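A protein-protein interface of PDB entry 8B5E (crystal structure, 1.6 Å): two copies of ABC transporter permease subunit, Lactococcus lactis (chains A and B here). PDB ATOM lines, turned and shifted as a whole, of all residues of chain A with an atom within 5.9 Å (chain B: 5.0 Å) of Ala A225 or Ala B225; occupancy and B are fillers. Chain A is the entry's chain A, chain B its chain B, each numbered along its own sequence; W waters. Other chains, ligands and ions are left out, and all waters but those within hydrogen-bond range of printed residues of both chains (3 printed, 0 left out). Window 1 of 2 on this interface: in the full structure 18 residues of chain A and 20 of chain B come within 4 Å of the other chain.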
ATOM      1  N   TYR A  86      13.742   5.450  -6.002  1.00  0.00           N
ATOM      2  CA  TYR A  86      14.206   5.988  -4.735  1.00  0.00           C
ATOM      3  C   TYR A  86      15.386   5.135  -4.295  1.00  0.00           C
ATOM      4  O   TYR A  86      15.343   3.920  -4.481  1.00  0.00           O
ATOM      5  CB  TYR A  86      13.116   5.934  -3.655  1.00  0.00           C
ATOM      6  CG  TYR A  86      13.535   6.560  -2.346  1.00  0.00           C
ATOM      7  CD1 TYR A  86      13.680   7.925  -2.222  1.00  0.00           C
ATOM      8  CD2 TYR A  86      13.858   5.792  -1.240  1.00  0.00           C
ATOM      9  CE1 TYR A  86      14.104   8.521  -1.043  1.00  0.00           C
ATOM     10  CE2 TYR A  86      14.282   6.364  -0.061  1.00  0.00           C
ATOM     11  CZ  TYR A  86      14.414   7.735   0.051  1.00  0.00           C
ATOM     12  OH  TYR A  86      14.862   8.328   1.228  1.00  0.00           O
ATOM     13  N   LYS A 209      10.004  13.442 -12.254  1.00  0.00           N
ATOM     14  CA  LYS A 209      11.237  14.025 -11.753  1.00  0.00           C
ATOM     15  C   LYS A 209      11.492  15.382 -12.417  1.00  0.00           C
ATOM     16  O   LYS A 209      12.006  16.297 -11.781  1.00  0.00           O
ATOM     17  CB  LYS A 209      12.433  13.097 -11.990  1.00  0.00           C
ATOM     18  CG  LYS A 209      12.602  11.931 -11.016  1.00  0.00           C
ATOM     19  CD  LYS A 209      13.768  11.067 -11.452  1.00  0.00           C
ATOM     20  CE  LYS A 209      14.245   9.987 -10.506  1.00  0.00           C
ATOM     21  NZ  LYS A 209      15.469   9.342 -11.061  1.00  0.00           N
ATOM     22  N   TYR A 214       7.515  14.534  -8.461  1.00  0.00           N
ATOM     23  CA  TYR A 214       8.235  13.531  -7.669  1.00  0.00           C
ATOM     24  C   TYR A 214       8.667  14.144  -6.336  1.00  0.00           C
ATOM     25  O   TYR A 214       8.387  13.582  -5.273  1.00  0.00           O
ATOM     26  CB  TYR A 214       9.426  12.981  -8.465  1.00  0.00           C
ATOM     27  CG  TYR A 214      10.390  12.098  -7.697  1.00  0.00           C
ATOM     28  CD1 TYR A 214      10.107  10.760  -7.485  1.00  0.00           C
ATOM     29  CD2 TYR A 214      11.580  12.596  -7.182  1.00  0.00           C
ATOM     30  CE1 TYR A 214      10.995   9.932  -6.820  1.00  0.00           C
ATOM     31  CE2 TYR A 214      12.471  11.791  -6.489  1.00  0.00           C
ATOM     32  CZ  TYR A 214      12.174  10.454  -6.312  1.00  0.00           C
ATOM     33  OH  TYR A 214      12.987   9.597  -5.639  1.00  0.00           O
ATOM     34  N   ASP A 215       9.298  15.335  -6.402  1.00  0.00           N
ATOM     35  CA  ASP A 215       9.771  16.032  -5.219  1.00  0.00           C
ATOM     36  C   ASP A 215       8.607  16.368  -4.285  1.00  0.00           C
ATOM     37  O   ASP A 215       8.729  16.293  -3.067  1.00  0.00           O
ATOM     38  CB  ASP A 215      10.540  17.306  -5.587  1.00  0.00           C
ATOM     39  CG  ASP A 215      10.906  18.170  -4.390  1.00  0.00           C
ATOM     40  OD1 ASP A 215      11.556  17.643  -3.457  1.00  0.00           O
ATOM     41  OD2 ASP A 215      10.516  19.364  -4.383  1.00  0.00           O
ATOM     42  N   LEU A 218       7.599  13.236  -2.223  1.00  0.00           N
ATOM     43  CA  LEU A 218       8.529  12.946  -1.131  1.00  0.00           C
ATOM     44  C   LEU A 218       8.339  13.930   0.030  1.00  0.00           C
ATOM     45  O   LEU A 218       8.296  13.555   1.209  1.00  0.00           O
ATOM     46  CB  LEU A 218       9.974  12.993  -1.649  1.00  0.00           C
ATOM     47  CG  LEU A 218      10.365  11.976  -2.720  1.00  0.00           C
ATOM     48  CD1 LEU A 218      11.866  11.855  -2.830  1.00  0.00           C
ATOM     49  CD2 LEU A 218       9.792  10.615  -2.471  1.00  0.00           C
ATOM     50  N   ILE A 223      10.573  13.696   3.420  1.00  0.00           N
ATOM     51  CA  ILE A 223      11.747  13.148   2.757  1.00  0.00           C
ATOM     52  C   ILE A 223      12.279  14.151   1.736  1.00  0.00           C
ATOM     53  O   ILE A 223      11.531  14.655   0.894  1.00  0.00           O
ATOM     54  CB  ILE A 223      11.367  11.804   2.108  1.00  0.00           C
ATOM     55  CG1 ILE A 223      10.980  10.826   3.217  1.00  0.00           C
ATOM     56  CG2 ILE A 223      12.479  11.243   1.216  1.00  0.00           C
ATOM     57  CD1 ILE A 223      10.090   9.762   2.738  1.00  0.00           C
ATOM     58  N   THR A 224      13.586  14.376   1.790  1.00  0.00           N
ATOM     59  CA  THR A 224      14.299  15.037   0.711  1.00  0.00           C
ATOM     60  C   THR A 224      14.760  13.988  -0.300  1.00  0.00           C
ATOM     61  O   THR A 224      15.368  12.977   0.064  1.00  0.00           O
ATOM     62  CB  THR A 224      15.495  15.836   1.229  1.00  0.00           C
ATOM     63  OG1 THR A 224      15.076  16.647   2.336  1.00  0.00           O
ATOM     64  CG2 THR A 224      16.115  16.678   0.130  1.00  0.00           C
ATOM     65  N   ALA A 225      14.472  14.256  -1.579  1.00  0.00           N
ATOM     66  CA  ALA A 225      14.968  13.446  -2.675  1.00  0.00           C
ATOM     67  C   ALA A 225      16.480  13.283  -2.502  1.00  0.00           C
ATOM     68  O   ALA A 225      17.144  14.339  -2.443  1.00  0.00           O
ATOM     69  CB  ALA A 225      14.631  14.108  -3.993  1.00  0.00           C
ATOM     70  OXT ALA A 225      16.934  12.121  -2.393  1.00  0.00           O
ATOM     71  N   TYR B  86      22.037  18.241   1.598  1.00  0.00           N
ATOM     72  CA  TYR B  86      21.377  17.753   0.395  1.00  0.00           C
ATOM     73  C   TYR B  86      22.013  16.396   0.045  1.00  0.00           C
ATOM     74  O   TYR B  86      23.163  16.141   0.382  1.00  0.00           O
ATOM     75  CB  TYR B  86      21.368  18.764  -0.786  1.00  0.00           C
ATOM     76  CG  TYR B  86      20.319  18.382  -1.816  1.00  0.00           C
ATOM     77  CD1 TYR B  86      18.977  18.338  -1.451  1.00  0.00           C
ATOM     78  CD2 TYR B  86      20.632  17.963  -3.104  1.00  0.00           C
ATOM     79  CE1 TYR B  86      17.990  17.903  -2.312  1.00  0.00           C
ATOM     80  CE2 TYR B  86      19.646  17.536  -3.993  1.00  0.00           C
ATOM     81  CZ  TYR B  86      18.316  17.492  -3.587  1.00  0.00           C
ATOM     82  OH  TYR B  86      17.228  17.067  -4.329  1.00  0.00           O
ATOM     83  N   THR B  87      21.216  15.507  -0.551  1.00  0.00           N
ATOM     84  CA  THR B  87      21.648  14.238  -1.104  1.00  0.00           C
ATOM     85  C   THR B  87      22.573  14.496  -2.293  1.00  0.00           C
ATOM     86  O   THR B  87      22.510  15.551  -2.946  1.00  0.00           O
ATOM     87  CB  THR B  87      20.443  13.356  -1.472  1.00  0.00           C
ATOM     88  OG1 THR B  87      19.694  14.003  -2.498  1.00  0.00           O
ATOM     89  CG2 THR B  87      19.513  13.061  -0.310  1.00  0.00           C
ATOM     90  N   VAL B 159      23.088  15.604  -9.910  1.00  0.00           N
ATOM     91  CA  VAL B 159      21.667  15.776 -10.163  1.00  0.00           C
ATOM     92  C   VAL B 159      21.292  17.249  -9.973  1.00  0.00           C
ATOM     93  O   VAL B 159      20.526  17.788 -10.787  1.00  0.00           O
ATOM     94  CB  VAL B 159      20.803  14.839  -9.290  1.00  0.00           C
ATOM     95  CG1 VAL B 159      19.362  15.323  -9.164  1.00  0.00           C
ATOM     96  CG2 VAL B 159      20.848  13.410  -9.796  1.00  0.00           C
ATOM     97  N   SER B 163      19.305  19.638 -12.634  1.00  0.00           N
ATOM     98  CA  SER B 163      18.005  20.167 -12.241  1.00  0.00           C
ATOM     99  C   SER B 163      17.950  21.679 -12.470  1.00  0.00           C
ATOM    100  O   SER B 163      16.949  22.204 -12.972  1.00  0.00           O
ATOM    101  CB  SER B 163      17.614  19.821 -10.802  1.00  0.00           C
ATOM    102  OG  SER B 163      17.302  18.445 -10.713  1.00  0.00           O
ATOM    103  N   MET B 174      15.415  14.183 -17.224  1.00  0.00           N
ATOM    104  CA  MET B 174      16.066  13.189 -16.377  1.00  0.00           C
ATOM    105  C   MET B 174      15.388  11.834 -16.560  1.00  0.00           C
ATOM    106  O   MET B 174      14.514  11.452 -15.787  1.00  0.00           O
ATOM    107  CB  MET B 174      16.018  13.626 -14.911  1.00  0.00           C
ATOM    108  CG  MET B 174      17.088  14.673 -14.610  1.00  0.00           C
ATOM    109  SD  MET B 174      17.107  15.252 -12.885  1.00  0.00           S
ATOM    110  CE  MET B 174      15.500  16.040 -12.823  1.00  0.00           C
ATOM    111  N   SER B 178      18.952   7.789 -10.718  1.00  0.00           N
ATOM    112  CA  SER B 178      19.890   8.542  -9.911  1.00  0.00           C
ATOM    113  C   SER B 178      20.812   7.521  -9.227  1.00  0.00           C
ATOM    114  O   SER B 178      20.333   6.498  -8.716  1.00  0.00           O
ATOM    115  CB  SER B 178      19.163   9.413  -8.904  1.00  0.00           C
ATOM    116  OG  SER B 178      18.483  10.532  -9.519  1.00  0.00           O
ATOM    117  N   ILE B 223      15.666  22.586  -7.747  1.00  0.00           N
ATOM    118  CA  ILE B 223      16.176  21.292  -7.304  1.00  0.00           C
ATOM    119  C   ILE B 223      14.993  20.405  -6.917  1.00  0.00           C
ATOM    120  O   ILE B 223      14.337  20.701  -5.917  1.00  0.00           O
ATOM    121  CB  ILE B 223      17.133  21.478  -6.098  1.00  0.00           C
ATOM    122  CG1 ILE B 223      18.161  22.588  -6.313  1.00  0.00           C
ATOM    123  CG2 ILE B 223      17.816  20.174  -5.699  1.00  0.00           C
ATOM    124  CD1 ILE B 223      18.895  22.537  -7.628  1.00  0.00           C
ATOM    125  N   THR B 224      14.704  19.370  -7.737  1.00  0.00           N
ATOM    126  CA  THR B 224      13.460  18.594  -7.664  1.00  0.00           C
ATOM    127  C   THR B 224      13.696  17.076  -7.558  1.00  0.00           C
ATOM    128  O   THR B 224      12.793  16.327  -7.173  1.00  0.00           O
ATOM    129  CB  THR B 224      12.554  18.897  -8.874  1.00  0.00           C
ATOM    130  OG1 THR B 224      13.260  18.527 -10.061  1.00  0.00           O
ATOM    131  CG2 THR B 224      12.132  20.350  -8.965  1.00  0.00           C
ATOM    132  N   ALA B 225      14.886  16.605  -7.950  1.00  0.00           N
ATOM    133  CA  ALA B 225      15.319  15.252  -7.640  1.00  0.00           C
ATOM    134  C   ALA B 225      16.722  15.303  -7.029  1.00  0.00           C
ATOM    135  O   ALA B 225      17.317  16.428  -6.976  1.00  0.00           O
ATOM    136  CB  ALA B 225      15.310  14.374  -8.871  1.00  0.00           C
ATOM    137  OXT ALA B 225      17.193  14.204  -6.669  1.00  0.00           O
HETATM  138  O   HOH W   1      14.416   9.014 -14.206  1.00  0.00           O
HETATM  139  O   HOH W   2      10.302  16.342  -8.945  1.00  0.00           O
HETATM  140  O   HOH W   3      16.406   6.947  -9.625  1.00  0.00           O
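The chain-end carboxylate of Ala A225 sits at hydrogen-bond distance from the side-chain hydroxyl of Thr B87, 2.6 Å away. The backbone carbonyl oxygen of Lys A209 lies within hydrogen-bond range of the side-chain hydroxyl of Thr B224 (3.1 Å). O of Ala A225 is in hydrogen-bond range of OH of Tyr B86, 3.3 Å away.
OH of Tyr B86 is in hydrogen-bond range of O of Ala B225 (2.7 Å).
CE of Met B174 touches O of Lys A209, at 3.7 Å. Ser B178 touches Lys A209 (OG to NZ, 3.6 Å). Tyr A214 touches Thr B224 (CD2 to O, 3.9 Å). CB of Asp A215 touches O of Thr B224 (2.9 Å). CE1 of Tyr B86 touches CG2 of Thr A224, 3.3 Å away. Ala A225 touches Ala B225.
Printed residues of chain B within 4 Å of Tyr A214: Thr B224. Of the printed residues of chain B, Asp A215 touches Thr B224 (2.9 Å). Ala A225 touches just these residues of chain B: Tyr B86, Thr B87 and Ala B225. Of the printed residues of chain A, Tyr B86 touches Thr A224 and Ala A225. Of the printed residues of chain A, Ser B178 touches Lys A209 (3.6 Å). Of the printed residues of chain A, Ala B225 touches Ala A225. The nearest printed residue of chain B that does not touch Lys A209 is Ala B225 (4.2 Å).
Hydrophobic or aromatic side chains of chain B that line the printed part of chain A: Tyr B86 and Met B174. Of the 8 printed residues of chain A, 5 touch a printed residue of chain B. Printed residues of chain A that touch a printed residue of chain B: Lys A209, Tyr A214, Asp A215, Thr A224 and Ala A225.
Thr A224 touches Tyr B86, but with the chains exchanged Tyr A86 does not touch Thr B224 (9.8 Å). Ala A225 touches Tyr B86, but with the chains exchanged Tyr A86 does not touch Ala B225 (8.5 Å). Ala A225 touches its own counterpart, Ala B225. Of the 9 pairs that touch across the chains among the printed residues, 1 has its exchanged pair printed and touching as well.
Water W3 lies within hydrogen-bond range of N of Ser B178 (2.9 Å) and NZ of Lys A209 (2.9 Å). Water W1 bridges O of Met B174 and NZ of Lys A209. Water W2 lies within hydrogen-bond range of the backbone NH of Asp A215 (2.9 Å), the backbone carbonyl oxygen of Thr B224 (3.1 Å), the backbone carbonyl oxygen of Lys A209 (3.3 Å) and the backbone NH of Tyr A214 (3.4 Å).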
